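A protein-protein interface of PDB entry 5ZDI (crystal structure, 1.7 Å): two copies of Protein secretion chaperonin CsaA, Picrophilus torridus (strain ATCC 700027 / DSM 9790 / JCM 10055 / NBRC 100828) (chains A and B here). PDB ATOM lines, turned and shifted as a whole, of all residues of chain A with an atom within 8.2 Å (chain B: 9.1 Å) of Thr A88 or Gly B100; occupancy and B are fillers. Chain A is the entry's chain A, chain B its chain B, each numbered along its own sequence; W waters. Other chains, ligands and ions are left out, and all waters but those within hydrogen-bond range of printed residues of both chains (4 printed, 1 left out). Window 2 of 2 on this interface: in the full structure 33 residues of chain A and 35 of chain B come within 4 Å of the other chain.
The backbone carbonyl oxygen (O) of Gly A85 lies within hydrogen-bond range of the backbone NH (N) of Ala B107.
The backbone carbonyl oxygen (O) of Lys B105 lies within hydrogen-bond range of the backbone NH (N) of Ile A87.
The backbone NH of Asp B98 is in hydrogen-bond range of the backbone carbonyl oxygen of Leu A94 (2.9 Å).
N of Ala A86 lies within hydrogen-bond range of O of Lys A93.
The side-chain carboxylate (OD2) of Asp A90 is in salt-bridge range of the side-chain amino group (NZ) of Lys A93 (3.0 Å).
The backbone NH (N) of Gly B103 sits at hydrogen-bond distance from the backbone carbonyl oxygen (O) of Val B14, at 2.7 Å.
The backbone carbonyl oxygen (O) of Asp B104 is in hydrogen-bond range of the backbone NH (N) of Val B14 (2.8 Å).
The side-chain amino group of Lys B62 sits at hydrogen-bond distance from the backbone carbonyl oxygen of Gly B100.
N of Glu B101 lies within hydrogen-bond range of OD2 of Asp B104.
Among the printed residues, pairs that only touch across the chains: Gly A85 with Ile B106 (3.4 Å), Ile A87 with Asp B104 (3.5 Å), Thr A88 with Asp B104 (3.5 Å), Thr A88 with Gly B100 (3.5 Å), Ala A86 with Lys B105 (3.6 Å), Lys A93 with Gly B99 (3.6 Å), Ile A87 with Ala B107 (3.7 Å), Leu A94 with Pro B97 (3.7 Å), Thr A88 with Gly B99 (3.8 Å), Ala A86 with Val B14 (3.8 Å), Ala A86 with Ile B106 (3.9 Å) and Leu A94 with Thr B96 (3.9 Å).
Of the printed residues of chain B, Gly A85 touches Ile B106 and Ala B107.
Printed residues of chain B within 4 Å of Ala A86: Val B14, Lys B105 and Ile B106.
Of chain B, only Gly B99, Gly B100 and Asp B104 come within 4 Å of Thr A88.
Of the printed residues of chain A, Asp B98 touches Leu A94.
Of chain A, only Thr A88 (3.8 Å) and Lys A93 (3.6 Å) come within 4 Å of Gly B99.
Gly B100 touches just one residue of chain A: Thr A88.
Of the printed residues of chain A, Ala B107 touches Gly A85 and Ile A87.
Printed residues of chain A that touch a printed residue of chain B: Gly A85, Ala A86, Ile A87, Thr A88, Lys A93 and Leu A94.
Hydrophobic or aromatic side chains of chain A within 4 Å of the printed part of chain B: Ala A86, Ile A87 and Leu A94.
Of the 20 printed residues of chain B, 10 touch a printed residue of chain A.
Printed residues of chain B that touch a printed residue of chain A: Val B14, Thr B96, Pro B97, Asp B98, Gly B99, Gly B100, Asp B104, Lys B105, Ile B106 and Ala B107.
Hydrophobic or aromatic side chains of chain B that line the printed part of chain A: Val B14, Ile B106 and Ala B107.
Among the printed residues, 15 pairs touch across the chains.
No position is printed for both chains.
Water W3 bridges OD2 of Asp B104 (2.6 Å) and N of Gly A89 (2.9 Å).
Water W2 lies within hydrogen-bond range of O of Ile A87 (2.8 Å) and N of Lys B105 (2.9 Å).
Water W4 bridges the side-chain hydroxyl (OG1) of Thr A88 (2.9 Å) and the backbone NH (N) of Gly B100 (3.3 Å).
Water W1 bridges O of Asp B98 and NZ of Lys A93.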
ATOM      1  N   ASN A  52     -18.854  -3.840  22.769  1.00  0.00           N
ATOM      2  CA  ASN A  52     -19.437  -3.454  24.030  1.00  0.00           C
ATOM      3  C   ASN A  52     -18.728  -4.002  25.236  1.00  0.00           C
ATOM      4  O   ASN A  52     -18.808  -3.431  26.349  1.00  0.00           O
ATOM      5  CB  ASN A  52     -20.959  -3.761  24.078  1.00  0.00           C
ATOM      6  CG  ASN A  52     -21.355  -5.218  23.611  1.00  0.00           C
ATOM      7  OD1 ASN A  52     -20.871  -5.716  22.544  1.00  0.00           O
ATOM      8  ND2 ASN A  52     -22.316  -5.868  24.377  1.00  0.00           N
ATOM      9  N   GLY A  85     -23.895 -15.229  20.517  1.00  0.00           N
ATOM     10  CA  GLY A  85     -24.410 -14.282  21.498  1.00  0.00           C
ATOM     11  C   GLY A  85     -25.834 -13.900  21.169  1.00  0.00           C
ATOM     12  O   GLY A  85     -26.226 -14.065  20.055  1.00  0.00           O
ATOM     13  N   ALA A  86     -26.560 -13.394  22.163  1.00  0.00           N
ATOM     14  CA  ALA A  86     -27.911 -12.919  22.020  1.00  0.00           C
ATOM     15  C   ALA A  86     -27.905 -11.471  21.558  1.00  0.00           C
ATOM     16  O   ALA A  86     -27.150 -10.658  22.040  1.00  0.00           O
ATOM     17  CB  ALA A  86     -28.635 -13.064  23.308  1.00  0.00           C
ATOM     18  N   ILE A  87     -28.807 -11.145  20.651  1.00  0.00           N
ATOM     19  CA  ILE A  87     -28.995  -9.721  20.219  1.00  0.00           C
ATOM     20  C   ILE A  87     -30.012  -9.095  21.114  1.00  0.00           C
ATOM     21  O   ILE A  87     -31.175  -9.526  21.180  1.00  0.00           O
ATOM     22  CB  ILE A  87     -29.533  -9.706  18.774  1.00  0.00           C
ATOM     23  CG1 ILE A  87     -28.533 -10.462  17.836  1.00  0.00           C
ATOM     24  CG2 ILE A  87     -29.778  -8.294  18.298  1.00  0.00           C
ATOM     25  CD1 ILE A  87     -29.006 -10.650  16.426  1.00  0.00           C
ATOM     26  N   THR A  88     -29.553  -8.164  21.899  1.00  0.00           N
ATOM     27  CA  THR A  88     -30.398  -7.625  22.964  1.00  0.00           C
ATOM     28  C   THR A  88     -30.549  -6.132  22.745  1.00  0.00           C
ATOM     29  O   THR A  88     -29.823  -5.537  21.968  1.00  0.00           O
ATOM     30  CB  THR A  88     -29.829  -7.825  24.371  1.00  0.00           C
ATOM     31  OG1 THR A  88     -28.793  -6.857  24.627  1.00  0.00           O
ATOM     32  CG2 THR A  88     -29.329  -9.287  24.543  1.00  0.00           C
ATOM     33  N   GLY A  89     -31.410  -5.541  23.563  1.00  0.00           N
ATOM     34  CA  GLY A  89     -31.577  -4.081  23.569  1.00  0.00           C
ATOM     35  C   GLY A  89     -30.332  -3.337  24.049  1.00  0.00           C
ATOM     36  O   GLY A  89     -30.191  -2.144  23.777  1.00  0.00           O
ATOM     37  N   ASP A  90     -29.415  -4.030  24.730  1.00  0.00           N
ATOM     38  CA  ASP A  90     -28.124  -3.459  25.194  1.00  0.00           C
ATOM     39  C   ASP A  90     -26.890  -4.023  24.374  1.00  0.00           C
ATOM     40  O   ASP A  90     -25.797  -4.120  24.909  1.00  0.00           O
ATOM     41  CB  ASP A  90     -28.051  -3.709  26.722  1.00  0.00           C
ATOM     42  CG  ASP A  90     -26.876  -2.969  27.443  1.00  0.00           C
ATOM     43  OD1 ASP A  90     -26.609  -1.797  27.064  1.00  0.00           O
ATOM     44  OD2 ASP A  90     -26.225  -3.557  28.396  1.00  0.00           O
ATOM     45  N   GLY A  91     -27.058  -4.320  23.072  1.00  0.00           N
ATOM     46  CA  GLY A  91     -26.044  -4.984  22.293  1.00  0.00           C
ATOM     47  C   GLY A  91     -25.964  -6.529  22.441  1.00  0.00           C
ATOM     48  O   GLY A  91     -26.812  -7.176  23.086  1.00  0.00           O
ATOM     49  N   VAL A  92     -24.936  -7.061  21.824  1.00  0.00           N
ATOM     50  CA  VAL A  92     -24.692  -8.474  21.806  1.00  0.00           C
ATOM     51  C   VAL A  92     -24.218  -8.901  23.203  1.00  0.00           C
ATOM     52  O   VAL A  92     -23.250  -8.403  23.707  1.00  0.00           O
ATOM     53  CB  VAL A  92     -23.687  -8.838  20.739  1.00  0.00           C
ATOM     54  CG1 VAL A  92     -23.338 -10.339  20.771  1.00  0.00           C
ATOM     55  CG2 VAL A  92     -24.247  -8.508  19.333  1.00  0.00           C
ATOM     56  N   LYS A  93     -24.857  -9.943  23.758  1.00  0.00           N
ATOM     57  CA  LYS A  93     -24.478 -10.483  25.057  1.00  0.00           C
ATOM     58  C   LYS A  93     -24.080 -11.935  24.819  1.00  0.00           C
ATOM     59  O   LYS A  93     -24.915 -12.787  24.459  1.00  0.00           O
ATOM     60  CB  LYS A  93     -25.640 -10.410  26.009  1.00  0.00           C
ATOM     61  CG  LYS A  93     -26.047  -8.992  26.337  1.00  0.00           C
ATOM     62  CD  LYS A  93     -25.063  -8.304  27.320  1.00  0.00           C
ATOM     63  CE  LYS A  93     -25.605  -6.929  27.663  1.00  0.00           C
ATOM     64  NZ  LYS A  93     -24.730  -6.182  28.541  1.00  0.00           N
ATOM     65  N   LEU A  94     -22.814 -12.214  25.053  1.00  0.00           N
ATOM     66  CA  LEU A  94     -22.284 -13.577  24.885  1.00  0.00           C
ATOM     67  C   LEU A  94     -23.057 -14.621  25.676  1.00  0.00           C
ATOM     68  O   LEU A  94     -23.449 -14.407  26.844  1.00  0.00           O
ATOM     69  CB  LEU A  94     -20.815 -13.688  25.286  1.00  0.00           C
ATOM     70  CG  LEU A  94     -19.901 -12.842  24.366  1.00  0.00           C
ATOM     71  CD1 LEU A  94     -18.522 -12.727  25.014  1.00  0.00           C
ATOM     72  CD2 LEU A  94     -19.886 -13.421  22.931  1.00  0.00           C
ATOM     73  N   ARG B  13     -33.343 -18.950  21.004  1.00  0.00           N
ATOM     74  CA  ARG B  13     -33.814 -17.825  21.787  1.00  0.00           C
ATOM     75  C   ARG B  13     -33.383 -17.876  23.262  1.00  0.00           C
ATOM     76  O   ARG B  13     -33.209 -18.964  23.836  1.00  0.00           O
ATOM     77  CB  ARG B  13     -35.325 -17.679  21.732  1.00  0.00           C
ATOM     78  CG  ARG B  13     -35.961 -17.498  20.329  1.00  0.00           C
ATOM     79  CD  ARG B  13     -35.473 -16.264  19.601  1.00  0.00           C
ATOM     80  NE  ARG B  13     -36.248 -16.306  18.362  1.00  0.00           N
ATOM     81  CZ  ARG B  13     -37.413 -15.690  18.161  1.00  0.00           C
ATOM     82  NH1 ARG B  13     -37.879 -14.749  19.059  1.00  0.00           N
ATOM     83  NH2 ARG B  13     -38.121 -16.003  17.022  1.00  0.00           N
ATOM     84  N   VAL B  14     -33.331 -16.694  23.865  1.00  0.00           N
ATOM     85  CA  VAL B  14     -33.306 -16.573  25.301  1.00  0.00           C
ATOM     86  C   VAL B  14     -34.674 -16.839  25.854  1.00  0.00           C
ATOM     87  O   VAL B  14     -35.704 -16.371  25.308  1.00  0.00           O
ATOM     88  CB  VAL B  14     -32.865 -15.199  25.735  1.00  0.00           C
ATOM     89  CG1 VAL B  14     -32.940 -15.093  27.271  1.00  0.00           C
ATOM     90  CG2 VAL B  14     -31.514 -14.829  25.136  1.00  0.00           C
ATOM     91  N   GLY B  15     -34.713 -17.714  26.836  1.00  0.00           N
ATOM     92  CA  GLY B  15     -35.940 -17.933  27.604  1.00  0.00           C
ATOM     93  C   GLY B  15     -35.706 -17.881  29.129  1.00  0.00           C
ATOM     94  O   GLY B  15     -34.552 -17.901  29.570  1.00  0.00           O
ATOM     95  N   ILE B  16     -36.765 -17.838  29.909  1.00  0.00           N
ATOM     96  CA  ILE B  16     -36.661 -17.866  31.392  1.00  0.00           C
ATOM     97  C   ILE B  16     -37.499 -18.966  32.001  1.00  0.00           C
ATOM     98  O   ILE B  16     -38.668 -19.128  31.699  1.00  0.00           O
ATOM     99  CB  ILE B  16     -36.916 -16.488  32.029  1.00  0.00           C
ATOM    100  CG1 ILE B  16     -36.647 -16.531  33.539  1.00  0.00           C
ATOM    101  CG2 ILE B  16     -38.297 -16.085  31.778  1.00  0.00           C
ATOM    102  CD1 ILE B  16     -36.403 -15.180  34.172  1.00  0.00           C
ATOM    103  N   LYS B  61     -34.091 -18.621  36.058  1.00  0.00           N
ATOM    104  CA  LYS B  61     -32.807 -18.685  35.322  1.00  0.00           C
ATOM    105  C   LYS B  61     -33.068 -18.428  33.815  1.00  0.00           C
ATOM    106  O   LYS B  61     -33.969 -19.076  33.198  1.00  0.00           O
ATOM    107  CB  LYS B  61     -32.145 -20.059  35.494  1.00  0.00           C
ATOM    108  CG  LYS B  61     -30.720 -20.108  35.015  1.00  0.00           C
ATOM    109  CD  LYS B  61     -30.147 -21.506  35.293  1.00  0.00           C
ATOM    110  CE  LYS B  61     -28.761 -21.677  34.671  1.00  0.00           C
ATOM    111  NZ  LYS B  61     -27.716 -20.934  35.362  1.00  0.00           N
ATOM    112  N   LYS B  62     -32.241 -17.571  33.220  1.00  0.00           N
ATOM    113  CA  LYS B  62     -32.296 -17.321  31.780  1.00  0.00           C
ATOM    114  C   LYS B  62     -31.504 -18.421  31.079  1.00  0.00           C
ATOM    115  O   LYS B  62     -30.302 -18.597  31.368  1.00  0.00           O
ATOM    116  CB  LYS B  62     -31.707 -15.954  31.446  1.00  0.00           C
ATOM    117  CG  LYS B  62     -32.530 -14.799  32.027  1.00  0.00           C
ATOM    118  CD  LYS B  62     -32.006 -13.481  31.534  1.00  0.00           C
ATOM    119  CE  LYS B  62     -32.592 -12.308  32.282  1.00  0.00           C
ATOM    120  NZ  LYS B  62     -31.911 -11.014  31.933  1.00  0.00           N
ATOM    121  N   ILE B  63     -32.136 -19.140  30.189  1.00  0.00           N
ATOM    122  CA  ILE B  63     -31.511 -20.204  29.448  1.00  0.00           C
ATOM    123  C   ILE B  63     -31.593 -19.889  27.934  1.00  0.00           C
ATOM    124  O   ILE B  63     -32.169 -18.860  27.514  1.00  0.00           O
ATOM    125  CB  ILE B  63     -32.188 -21.563  29.826  1.00  0.00           C
ATOM    126  CG1 ILE B  63     -33.667 -21.572  29.633  1.00  0.00           C
ATOM    127  CG2 ILE B  63     -31.874 -21.839  31.278  1.00  0.00           C
ATOM    128  CD1 ILE B  63     -34.124 -21.654  28.202  1.00  0.00           C
ATOM    129  N   ILE B  64     -31.020 -20.791  27.149  1.00  0.00           N
ATOM    130  CA  ILE B  64     -30.991 -20.676  25.749  1.00  0.00           C
ATOM    131  C   ILE B  64     -31.640 -21.895  25.174  1.00  0.00           C
ATOM    132  O   ILE B  64     -31.298 -23.012  25.546  1.00  0.00           O
ATOM    133  CB  ILE B  64     -29.488 -20.620  25.267  1.00  0.00           C
ATOM    134  CG1 ILE B  64     -28.730 -19.457  25.939  1.00  0.00           C
ATOM    135  CG2 ILE B  64     -29.374 -20.503  23.765  1.00  0.00           C
ATOM    136  CD1 ILE B  64     -29.365 -18.093  25.758  1.00  0.00           C
ATOM    137  N   THR B  96     -26.142 -19.845  29.606  1.00  0.00           N
ATOM    138  CA  THR B  96     -26.860 -18.615  29.943  1.00  0.00           C
ATOM    139  C   THR B  96     -26.355 -17.426  29.131  1.00  0.00           C
ATOM    140  O   THR B  96     -25.164 -17.345  28.786  1.00  0.00           O
ATOM    141  CB  THR B  96     -26.795 -18.248  31.434  1.00  0.00           C
ATOM    142  OG1 THR B  96     -25.515 -17.693  31.744  1.00  0.00           O
ATOM    143  CG2 THR B  96     -27.081 -19.532  32.235  1.00  0.00           C
ATOM    144  N   PRO B  97     -27.252 -16.472  28.836  1.00  0.00           N
ATOM    145  CA  PRO B  97     -26.750 -15.248  28.281  1.00  0.00           C
ATOM    146  C   PRO B  97     -26.175 -14.264  29.323  1.00  0.00           C
ATOM    147  O   PRO B  97     -26.670 -14.210  30.400  1.00  0.00           O
ATOM    148  CB  PRO B  97     -27.996 -14.656  27.629  1.00  0.00           C
ATOM    149  CG  PRO B  97     -29.113 -15.046  28.505  1.00  0.00           C
ATOM    150  CD  PRO B  97     -28.712 -16.422  29.008  1.00  0.00           C
ATOM    151  N   ASP B  98     -25.200 -13.426  28.955  1.00  0.00           N
ATOM    152  CA  ASP B  98     -24.692 -12.453  29.865  1.00  0.00           C
ATOM    153  C   ASP B  98     -25.801 -11.412  30.180  1.00  0.00           C
ATOM    154  O   ASP B  98     -25.727 -10.770  31.237  1.00  0.00           O
ATOM    155  CB  ASP B  98     -23.448 -11.728  29.319  1.00  0.00           C
ATOM    156  CG  ASP B  98     -22.160 -12.518  29.464  1.00  0.00           C
ATOM    157  OD1 ASP B  98     -22.142 -13.557  30.157  1.00  0.00           O
ATOM    158  OD2 ASP B  98     -21.157 -12.144  28.800  1.00  0.00           O
ATOM    159  N   GLY B  99     -26.815 -11.266  29.305  1.00  0.00           N
ATOM    160  CA  GLY B  99     -27.964 -10.412  29.566  1.00  0.00           C
ATOM    161  C   GLY B  99     -28.988 -10.681  28.480  1.00  0.00           C
ATOM    162  O   GLY B  99     -28.708 -11.457  27.549  1.00  0.00           O
ATOM    163  N   GLY B 100     -30.140 -10.012  28.518  1.00  0.00           N
ATOM    164  CA  GLY B 100     -31.086 -10.242  27.465  1.00  0.00           C
ATOM    165  C   GLY B 100     -32.447 -10.531  28.073  1.00  0.00           C
ATOM    166  O   GLY B 100     -32.590 -10.805  29.268  1.00  0.00           O
ATOM    167  N   GLU B 101     -33.431 -10.427  27.237  1.00  0.00           N
ATOM    168  CA  GLU B 101     -34.812 -10.683  27.616  1.00  0.00           C
ATOM    169  C   GLU B 101     -35.328 -11.914  26.899  1.00  0.00           C
ATOM    170  O   GLU B 101     -34.886 -12.256  25.787  1.00  0.00           O
ATOM    171  CB  GLU B 101     -35.708  -9.443  27.242  1.00  0.00           C
ATOM    172  CG  GLU B 101     -35.335  -8.191  27.998  1.00  0.00           C
ATOM    173  CD  GLU B 101     -35.519  -8.288  29.543  1.00  0.00           C
ATOM    174  OE1 GLU B 101     -36.241  -9.125  30.129  1.00  0.00           O
ATOM    175  OE2 GLU B 101     -34.871  -7.511  30.216  1.00  0.00           O
ATOM    176  N   PRO B 102     -36.295 -12.602  27.521  1.00  0.00           N
ATOM    177  CA  PRO B 102     -36.973 -13.703  26.847  1.00  0.00           C
ATOM    178  C   PRO B 102     -37.477 -13.347  25.464  1.00  0.00           C
ATOM    179  O   PRO B 102     -38.078 -12.263  25.284  1.00  0.00           O
ATOM    180  CB  PRO B 102     -38.126 -13.999  27.842  1.00  0.00           C
ATOM    181  CG  PRO B 102     -37.570 -13.710  29.152  1.00  0.00           C
ATOM    182  CD  PRO B 102     -36.731 -12.465  28.919  1.00  0.00           C
ATOM    183  N   GLY B 103     -37.147 -14.196  24.474  1.00  0.00           N
ATOM    184  CA  GLY B 103     -37.433 -13.957  23.035  1.00  0.00           C
ATOM    185  C   GLY B 103     -36.323 -13.331  22.291  1.00  0.00           C
ATOM    186  O   GLY B 103     -36.337 -13.367  21.054  1.00  0.00           O
ATOM    187  N   ASP B 104     -35.301 -12.829  23.005  1.00  0.00           N
ATOM    188  CA  ASP B 104     -34.075 -12.296  22.259  1.00  0.00           C
ATOM    189  C   ASP B 104     -33.413 -13.435  21.485  1.00  0.00           C
ATOM    190  O   ASP B 104     -33.332 -14.570  22.005  1.00  0.00           O
ATOM    191  CB  ASP B 104     -33.062 -11.639  23.201  1.00  0.00           C
ATOM    192  CG  ASP B 104     -33.499 -10.261  23.696  1.00  0.00           C
ATOM    193  OD1 ASP B 104     -34.554  -9.786  23.198  1.00  0.00           O
ATOM    194  OD2 ASP B 104     -32.813  -9.702  24.594  1.00  0.00           O
ATOM    195  N   LYS B 105     -32.949 -13.137  20.266  1.00  0.00           N
ATOM    196  CA  LYS B 105     -32.464 -14.158  19.308  1.00  0.00           C
ATOM    197  C   LYS B 105     -30.949 -14.200  19.253  1.00  0.00           C
ATOM    198  O   LYS B 105     -30.253 -13.175  19.317  1.00  0.00           O
ATOM    199  CB  LYS B 105     -33.004 -13.822  17.910  1.00  0.00           C
ATOM    200  CG  LYS B 105     -32.811 -14.908  16.909  1.00  0.00           C
ATOM    201  CD  LYS B 105     -33.683 -14.656  15.639  1.00  0.00           C
ATOM    202  CE  LYS B 105     -33.162 -15.490  14.419  1.00  0.00           C
ATOM    203  NZ  LYS B 105     -33.203 -16.961  14.675  1.00  0.00           N
ATOM    204  N   ILE B 106     -30.431 -15.413  19.111  1.00  0.00           N
ATOM    205  CA  ILE B 106     -29.019 -15.609  18.983  1.00  0.00           C
ATOM    206  C   ILE B 106     -28.626 -15.317  17.571  1.00  0.00           C
ATOM    207  O   ILE B 106     -29.249 -15.830  16.638  1.00  0.00           O
ATOM    208  CB  ILE B 106     -28.629 -17.004  19.509  1.00  0.00           C
ATOM    209  CG1 ILE B 106     -28.541 -16.965  21.062  1.00  0.00           C
ATOM    210  CG2 ILE B 106     -27.319 -17.475  18.860  1.00  0.00           C
ATOM    211  CD1 ILE B 106     -29.727 -16.521  21.894  1.00  0.00           C
ATOM    212  N   ALA B 107     -27.551 -14.539  17.398  1.00  0.00           N
ATOM    213  CA  ALA B 107     -27.142 -14.064  16.114  1.00  0.00           C
ATOM    214  C   ALA B 107     -26.515 -15.086  15.236  1.00  0.00           C
ATOM    215  O   ALA B 107     -25.757 -15.984  15.672  1.00  0.00           O
ATOM    216  CB  ALA B 107     -26.133 -12.910  16.267  1.00  0.00           C
ATOM    217  OXT ALA B 107     -26.711 -14.923  13.980  1.00  0.00           O
HETATM  218  O   HOH W   1     -25.527  -7.840  30.938  1.00  0.00           O
HETATM  219  O   HOH W   2     -33.081 -10.410  19.281  1.00  0.00           O
HETATM  220  O   HOH W   3     -33.225  -7.227  25.105  1.00  0.00           O
HETATM  221  O   HOH W   4     -28.971  -7.091  27.537  1.00  0.00           O
